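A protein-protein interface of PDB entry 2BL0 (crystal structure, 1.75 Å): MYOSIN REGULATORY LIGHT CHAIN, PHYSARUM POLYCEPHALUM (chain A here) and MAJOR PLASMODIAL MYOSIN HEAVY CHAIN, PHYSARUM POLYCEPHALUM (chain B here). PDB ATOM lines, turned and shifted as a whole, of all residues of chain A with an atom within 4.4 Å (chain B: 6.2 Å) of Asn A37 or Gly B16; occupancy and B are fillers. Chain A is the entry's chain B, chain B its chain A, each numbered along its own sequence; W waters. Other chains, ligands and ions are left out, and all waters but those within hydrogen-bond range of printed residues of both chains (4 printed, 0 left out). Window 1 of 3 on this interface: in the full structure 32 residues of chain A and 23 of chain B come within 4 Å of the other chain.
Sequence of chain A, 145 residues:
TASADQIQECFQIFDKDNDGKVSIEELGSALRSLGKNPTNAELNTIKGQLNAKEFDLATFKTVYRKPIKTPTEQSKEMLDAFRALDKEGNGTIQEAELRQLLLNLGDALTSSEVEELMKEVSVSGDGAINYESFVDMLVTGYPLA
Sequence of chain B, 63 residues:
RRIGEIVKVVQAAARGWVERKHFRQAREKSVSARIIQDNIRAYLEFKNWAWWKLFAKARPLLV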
ATOM      1  N   ARG A  32      17.691  19.067   3.746  1.00  0.00           N
ATOM      2  CA  ARG A  32      18.961  19.300   3.091  1.00  0.00           C
ATOM      3  C   ARG A  32      20.149  18.745   3.895  1.00  0.00           C
ATOM      4  O   ARG A  32      21.106  18.244   3.316  1.00  0.00           O
ATOM      5  CB  ARG A  32      19.134  20.787   2.845  1.00  0.00           C
ATOM      6  CG  ARG A  32      18.240  21.290   1.748  1.00  0.00           C
ATOM      7  CD  ARG A  32      18.072  22.799   1.711  1.00  0.00           C
ATOM      8  NE  ARG A  32      17.091  23.145   0.689  1.00  0.00           N
ATOM      9  CZ  ARG A  32      16.178  24.104   0.783  1.00  0.00           C
ATOM     10  NH1 ARG A  32      16.088  24.894   1.860  1.00  0.00           N
ATOM     11  NH2 ARG A  32      15.322  24.262  -0.206  1.00  0.00           N
ATOM     12  N   GLY A  35      20.762  15.200   2.888  1.00  0.00           N
ATOM     13  CA  GLY A  35      21.076  14.869   1.516  1.00  0.00           C
ATOM     14  C   GLY A  35      19.938  14.805   0.522  1.00  0.00           C
ATOM     15  O   GLY A  35      20.062  14.140  -0.517  1.00  0.00           O
ATOM     16  N   LYS A  36      18.845  15.495   0.806  1.00  0.00           N
ATOM     17  CA  LYS A  36      17.803  15.702  -0.179  1.00  0.00           C
ATOM     18  C   LYS A  36      17.580  17.206  -0.404  1.00  0.00           C
ATOM     19  O   LYS A  36      17.543  18.000   0.525  1.00  0.00           O
ATOM     20  CB  LYS A  36      16.530  14.979   0.233  1.00  0.00           C
ATOM     21  CG  LYS A  36      16.639  13.484   0.017  1.00  0.00           C
ATOM     22  CD  LYS A  36      15.370  12.725   0.333  1.00  0.00           C
ATOM     23  CE  LYS A  36      15.663  11.212   0.357  1.00  0.00           C
ATOM     24  NZ  LYS A  36      14.426  10.349   0.125  1.00  0.00           N
ATOM     25  N   ASN A  37      17.444  17.578  -1.669  1.00  0.00           N
ATOM     26  CA  ASN A  37      17.531  18.965  -2.131  1.00  0.00           C
ATOM     27  C   ASN A  37      16.254  19.450  -2.839  1.00  0.00           C
ATOM     28  O   ASN A  37      16.219  19.564  -4.061  1.00  0.00           O
ATOM     29  CB  ASN A  37      18.664  19.100  -3.148  1.00  0.00           C
ATOM     30  CG  ASN A  37      20.043  18.909  -2.551  1.00  0.00           C
ATOM     31  OD1 ASN A  37      20.224  18.901  -1.327  1.00  0.00           O
ATOM     32  ND2 ASN A  37      21.041  18.748  -3.436  1.00  0.00           N
ATOM     33  N   PRO A  38      15.221  19.805  -2.084  1.00  0.00           N
ATOM     34  CA  PRO A  38      14.021  20.351  -2.700  1.00  0.00           C
ATOM     35  C   PRO A  38      14.292  21.734  -3.269  1.00  0.00           C
ATOM     36  O   PRO A  38      15.041  22.521  -2.681  1.00  0.00           O
ATOM     37  CB  PRO A  38      13.040  20.449  -1.526  1.00  0.00           C
ATOM     38  CG  PRO A  38      13.879  20.574  -0.373  1.00  0.00           C
ATOM     39  CD  PRO A  38      15.127  19.785  -0.617  1.00  0.00           C
ATOM     40  N   THR A  39      13.647  22.041  -4.379  1.00  0.00           N
ATOM     41  CA  THR A  39      13.615  23.416  -4.863  1.00  0.00           C
ATOM     42  C   THR A  39      12.653  24.173  -3.963  1.00  0.00           C
ATOM     43  O   THR A  39      11.912  23.559  -3.191  1.00  0.00           O
ATOM     44  CB  THR A  39      13.151  23.492  -6.303  1.00  0.00           C
ATOM     45  OG1 THR A  39      11.781  23.073  -6.399  1.00  0.00           O
ATOM     46  CG2 THR A  39      13.941  22.528  -7.200  1.00  0.00           C
ATOM     47  N   GLU A  42       9.073  23.015  -4.686  1.00  0.00           N
ATOM     48  CA  GLU A  42       8.785  21.713  -4.120  1.00  0.00           C
ATOM     49  C   GLU A  42       8.571  21.832  -2.627  1.00  0.00           C
ATOM     50  O   GLU A  42       7.623  21.269  -2.066  1.00  0.00           O
ATOM     51  CB  GLU A  42       9.924  20.742  -4.422  1.00  0.00           C
ATOM     52  CG  GLU A  42       9.957  20.348  -5.888  1.00  0.00           C
ATOM     53  CD  GLU A  42      11.260  19.693  -6.334  1.00  0.00           C
ATOM     54  OE1 GLU A  42      12.234  19.612  -5.548  1.00  0.00           O
ATOM     55  OE2 GLU A  42      11.299  19.282  -7.527  1.00  0.00           O
ATOM     56  N   ILE A  68      12.344  13.095  -3.067  1.00  0.00           N
ATOM     57  CA  ILE A  68      12.988  14.380  -3.255  1.00  0.00           C
ATOM     58  C   ILE A  68      14.393  14.089  -3.796  1.00  0.00           C
ATOM     59  O   ILE A  68      15.063  13.179  -3.322  1.00  0.00           O
ATOM     60  CB  ILE A  68      13.043  15.133  -1.908  1.00  0.00           C
ATOM     61  CG1 ILE A  68      11.629  15.332  -1.326  1.00  0.00           C
ATOM     62  CG2 ILE A  68      13.741  16.460  -2.093  1.00  0.00           C
ATOM     63  CD1 ILE A  68      11.598  15.809   0.145  1.00  0.00           C
ATOM     64  N   LYS A  69      14.831  14.861  -4.787  1.00  0.00           N
ATOM     65  CA  LYS A  69      16.113  14.616  -5.442  1.00  0.00           C
ATOM     66  C   LYS A  69      17.310  14.691  -4.503  1.00  0.00           C
ATOM     67  O   LYS A  69      17.429  15.629  -3.709  1.00  0.00           O
ATOM     68  CB  LYS A  69      16.326  15.620  -6.588  1.00  0.00           C
ATOM     69  CG  LYS A  69      15.380  15.433  -7.776  1.00  0.00           C
ATOM     70  CD  LYS A  69      16.051  15.756  -9.082  1.00  0.00           C
ATOM     71  CE  LYS A  69      15.061  15.848 -10.225  1.00  0.00           C
ATOM     72  NZ  LYS A  69      15.365  17.050 -11.040  1.00  0.00           N
ATOM     73  N   PRO A  71      21.621  14.935  -4.426  1.00  0.00           N
ATOM     74  CA  PRO A  71      22.553  15.715  -5.248  1.00  0.00           C
ATOM     75  C   PRO A  71      22.981  15.029  -6.564  1.00  0.00           C
ATOM     76  O   PRO A  71      23.044  15.714  -7.576  1.00  0.00           O
ATOM     77  CB  PRO A  71      23.731  15.956  -4.299  1.00  0.00           C
ATOM     78  CG  PRO A  71      23.128  15.877  -2.940  1.00  0.00           C
ATOM     79  CD  PRO A  71      22.119  14.771  -3.050  1.00  0.00           C
ATOM     80  N   GLN A  74      20.770  15.554  -9.466  1.00  0.00           N
ATOM     81  CA  GLN A  74      20.783  16.905 -10.032  1.00  0.00           C
ATOM     82  C   GLN A  74      21.982  17.203 -10.935  1.00  0.00           C
ATOM     83  O   GLN A  74      22.025  18.258 -11.546  1.00  0.00           O
ATOM     84  CB  GLN A  74      20.691  17.951  -8.921  1.00  0.00           C
ATOM     85  CG  GLN A  74      19.386  17.835  -8.135  1.00  0.00           C
ATOM     86  CD  GLN A  74      19.312  18.726  -6.922  1.00  0.00           C
ATOM     87  OE1 GLN A  74      20.288  18.840  -6.178  1.00  0.00           O
ATOM     88  NE2 GLN A  74      18.150  19.352  -6.706  1.00  0.00           N
ATOM     89  N   GLN B  11      20.669  26.354  -7.540  1.00  0.00           N
ATOM     90  CA  GLN B  11      20.332  26.930  -6.233  1.00  0.00           C
ATOM     91  C   GLN B  11      19.906  25.886  -5.195  1.00  0.00           C
ATOM     92  O   GLN B  11      20.292  25.959  -4.016  1.00  0.00           O
ATOM     93  CB  GLN B  11      19.285  28.012  -6.385  1.00  0.00           C
ATOM     94  CG  GLN B  11      19.858  29.218  -7.167  1.00  0.00           C
ATOM     95  CD  GLN B  11      18.788  30.149  -7.681  1.00  0.00           C
ATOM     96  OE1 GLN B  11      17.722  29.702  -8.086  1.00  0.00           O
ATOM     97  NE2 GLN B  11      19.070  31.443  -7.673  1.00  0.00           N
ATOM     98  N   ALA B  12      19.136  24.902  -5.639  1.00  0.00           N
ATOM     99  CA  ALA B  12      18.690  23.844  -4.750  1.00  0.00           C
ATOM    100  C   ALA B  12      19.879  23.030  -4.298  1.00  0.00           C
ATOM    101  O   ALA B  12      19.999  22.678  -3.134  1.00  0.00           O
ATOM    102  CB  ALA B  12      17.650  22.968  -5.437  1.00  0.00           C
ATOM    103  N   ALA B  13      20.805  22.744  -5.210  1.00  0.00           N
ATOM    104  CA  ALA B  13      21.935  21.900  -4.837  1.00  0.00           C
ATOM    105  C   ALA B  13      22.918  22.691  -3.976  1.00  0.00           C
ATOM    106  O   ALA B  13      23.570  22.129  -3.096  1.00  0.00           O
ATOM    107  CB  ALA B  13      22.605  21.343  -6.059  1.00  0.00           C
ATOM    108  N   ALA B  14      22.973  24.005  -4.208  1.00  0.00           N
ATOM    109  CA  ALA B  14      23.845  24.900  -3.439  1.00  0.00           C
ATOM    110  C   ALA B  14      23.364  25.003  -1.995  1.00  0.00           C
ATOM    111  O   ALA B  14      24.150  24.875  -1.058  1.00  0.00           O
ATOM    112  CB  ALA B  14      23.884  26.278  -4.076  1.00  0.00           C
ATOM    113  N   ARG B  15      22.065  25.207  -1.808  1.00  0.00           N
ATOM    114  CA  ARG B  15      21.495  25.176  -0.465  1.00  0.00           C
ATOM    115  C   ARG B  15      21.777  23.857   0.221  1.00  0.00           C
ATOM    116  O   ARG B  15      22.092  23.816   1.411  1.00  0.00           O
ATOM    117  CB  ARG B  15      19.985  25.384  -0.517  1.00  0.00           C
ATOM    118  CG  ARG B  15      19.570  26.802  -0.727  1.00  0.00           C
ATOM    119  CD  ARG B  15      18.042  26.988  -0.672  1.00  0.00           C
ATOM    120  NE  ARG B  15      17.707  28.403  -0.707  1.00  0.00           N
ATOM    121  CZ  ARG B  15      17.468  29.088  -1.821  1.00  0.00           C
ATOM    122  NH1 ARG B  15      17.415  28.484  -3.003  1.00  0.00           N
ATOM    123  NH2 ARG B  15      17.226  30.387  -1.745  1.00  0.00           N
ATOM    124  N   GLY B  16      21.657  22.764  -0.519  1.00  0.00           N
ATOM    125  CA  GLY B  16      21.936  21.465   0.041  1.00  0.00           C
ATOM    126  C   GLY B  16      23.333  21.402   0.605  1.00  0.00           C
ATOM    127  O   GLY B  16      23.533  20.950   1.725  1.00  0.00           O
ATOM    128  N   TRP B  17      24.325  21.806  -0.181  1.00  0.00           N
ATOM    129  CA  TRP B  17      25.715  21.779   0.263  1.00  0.00           C
ATOM    130  C   TRP B  17      25.947  22.650   1.514  1.00  0.00           C
ATOM    131  O   TRP B  17      26.575  22.215   2.471  1.00  0.00           O
ATOM    132  CB  TRP B  17      26.614  22.222  -0.899  1.00  0.00           C
ATOM    133  CG  TRP B  17      28.067  22.217  -0.612  1.00  0.00           C
ATOM    134  CD1 TRP B  17      28.938  21.181  -0.782  1.00  0.00           C
ATOM    135  CD2 TRP B  17      28.836  23.321  -0.133  1.00  0.00           C
ATOM    136  NE1 TRP B  17      30.204  21.577  -0.427  1.00  0.00           N
ATOM    137  CE2 TRP B  17      30.168  22.886  -0.018  1.00  0.00           C
ATOM    138  CE3 TRP B  17      28.520  24.636   0.252  1.00  0.00           C
ATOM    139  CZ2 TRP B  17      31.189  23.718   0.441  1.00  0.00           C
ATOM    140  CZ3 TRP B  17      29.524  25.463   0.712  1.00  0.00           C
ATOM    141  CH2 TRP B  17      30.852  25.003   0.792  1.00  0.00           C
ATOM    142  N   VAL B  18      25.375  23.845   1.535  1.00  0.00           N
ATOM    143  CA  VAL B  18      25.543  24.727   2.678  1.00  0.00           C
ATOM    144  C   VAL B  18      24.978  24.066   3.935  1.00  0.00           C
ATOM    145  O   VAL B  18      25.642  24.057   4.969  1.00  0.00           O
ATOM    146  CB  VAL B  18      24.918  26.111   2.441  1.00  0.00           C
ATOM    147  CG1 VAL B  18      25.056  26.986   3.684  1.00  0.00           C
ATOM    148  CG2 VAL B  18      25.615  26.807   1.290  1.00  0.00           C
ATOM    149  N   GLU B  19      23.792  23.477   3.834  1.00  0.00           N
ATOM    150  CA  GLU B  19      23.161  22.836   4.981  1.00  0.00           C
ATOM    151  C   GLU B  19      23.926  21.579   5.438  1.00  0.00           C
ATOM    152  O   GLU B  19      24.039  21.332   6.656  1.00  0.00           O
ATOM    153  CB  GLU B  19      21.699  22.475   4.695  1.00  0.00           C
ATOM    154  CG  GLU B  19      20.783  23.659   4.417  1.00  0.00           C
ATOM    155  CD  GLU B  19      20.605  24.596   5.606  1.00  0.00           C
ATOM    156  OE1 GLU B  19      21.028  24.266   6.732  1.00  0.00           O
ATOM    157  OE2 GLU B  19      20.010  25.682   5.385  1.00  0.00           O
ATOM    158  N   ARG B  20      24.463  20.804   4.490  1.00  0.00           N
ATOM    159  CA  ARG B  20      25.200  19.587   4.828  1.00  0.00           C
ATOM    160  C   ARG B  20      26.473  19.975   5.552  1.00  0.00           C
ATOM    161  O   ARG B  20      26.887  19.295   6.496  1.00  0.00           O
ATOM    162  CB  ARG B  20      25.571  18.743   3.589  1.00  0.00           C
ATOM    163  CG  ARG B  20      24.388  17.984   2.956  1.00  0.00           C
ATOM    164  CD  ARG B  20      24.803  16.815   2.079  1.00  0.00           C
ATOM    165  NE  ARG B  20      25.833  17.212   1.129  1.00  0.00           N
ATOM    166  CZ  ARG B  20      25.606  17.883  -0.007  1.00  0.00           C
ATOM    167  NH1 ARG B  20      24.387  18.235  -0.350  1.00  0.00           N
ATOM    168  NH2 ARG B  20      26.599  18.206  -0.811  1.00  0.00           N
ATOM    169  N   LYS B  21      27.077  21.076   5.107  1.00  0.00           N
ATOM    170  CA  LYS B  21      28.271  21.631   5.754  1.00  0.00           C
ATOM    171  C   LYS B  21      27.969  22.047   7.199  1.00  0.00           C
ATOM    172  O   LYS B  21      28.701  21.687   8.134  1.00  0.00           O
ATOM    173  CB  LYS B  21      28.796  22.830   4.975  1.00  0.00           C
ATOM    174  CG  LYS B  21      29.984  23.520   5.653  1.00  0.00           C
ATOM    175  CD  LYS B  21      30.706  24.467   4.715  1.00  0.00           C
ATOM    176  CE  LYS B  21      31.956  25.060   5.377  1.00  0.00           C
ATOM    177  NZ  LYS B  21      31.631  26.378   6.005  1.00  0.00           N
HETATM  178  O   HOH W   1      21.728  17.901   0.623  1.00  0.00           O
HETATM  179  O   HOH W   2      23.949  19.542  -2.966  1.00  0.00           O
HETATM  180  O   HOH W   3      18.385  25.734   3.465  1.00  0.00           O
HETATM  181  O   HOH W   4      17.684  22.149  -1.842  1.00  0.00           O
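Water W3 lies within hydrogen-bond range of OE2 of Glu B19 (2.5 Å) and NH1 of Arg A32 (2.9 Å).
Water W2 lies within hydrogen-bond range of the backbone carbonyl oxygen of Ala B13, the guanidinium group of Arg B20 and the side-chain amide nitrogen of Asn A37.
Water W1 lies within hydrogen-bond range of OD1 of Asn A37, O of Arg A32 and NH1 of Arg B20.
Water W4 lies within hydrogen-bond range of O of Ala B12 (2.7 Å), NE of Arg A32 (2.8 Å) and O of Pro A38 (2.8 Å).
Of chain B, only Ala B12, Ala B13 and Gly B16 come within 4 Å of Asn A37.
Of the printed residues of chain A, Arg B15 touches Arg A32.
Of the printed residues of chain A, Glu B19 touches Arg A32.
Of the printed residues of chain A, Arg B20 touches Arg A32 (3.3 Å) and Pro A71 (3.7 Å).
The nearest residue of chain B that does not touch Asn A37 is Arg B20 (4.3 Å).
The nearest printed residue of chain A that does not touch Gly B16 is Lys A36 (5.6 Å).
Of the 11 printed residues of chain A, 5 touch a printed residue of chain B.
Hydrophobic or aromatic side chains of chain A within 4 Å of the printed part of chain B: Pro A71.
Printed residues of chain B that touch a printed residue of chain A: Ala B12, Ala B13, Arg B15, Gly B16, Glu B19 and Arg B20.
Among the printed residues, 11 pairs touch across the chains.
Among the printed residues, no Asp or Glu carboxylate lies within 4 Å of a Lys or Arg side-chain nitrogen of the other chain.
NH2 of Arg A32 sits at hydrogen-bond distance from O of Pro A38, 3.0 Å away.
The backbone NH (N) of Asn A37 lies within hydrogen-bond range of the backbone carbonyl oxygen (O) of Lys A69 (2.8 Å).
ND2 of Asn A37 is in hydrogen-bond range of OE1 of Gln A74, 2.8 Å away.
O of Gly B16 touches O of Arg A32, 3.97 Å away.
CB of Arg A32 touches CB of Glu B19 (3.6 Å).
Arg A32 touches Arg B20 (O to CG, 3.3 Å).
Ala B12 touches Asn A37.
Asn A37 touches Ala B13 (ND2 to CA, 3.6 Å).
CA of Gly B16 touches OD1 of Asn A37, 3.4 Å away.
Ala B12 touches Pro A38.
Arg B20 touches Pro A71 (NH1 to CG, 3.7 Å).
CB of Ala B12 touches NE2 of Gln A74, at 3.9 Å.
Gln A74 touches Ala B13 (OE1 to CB, 3.4 Å).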
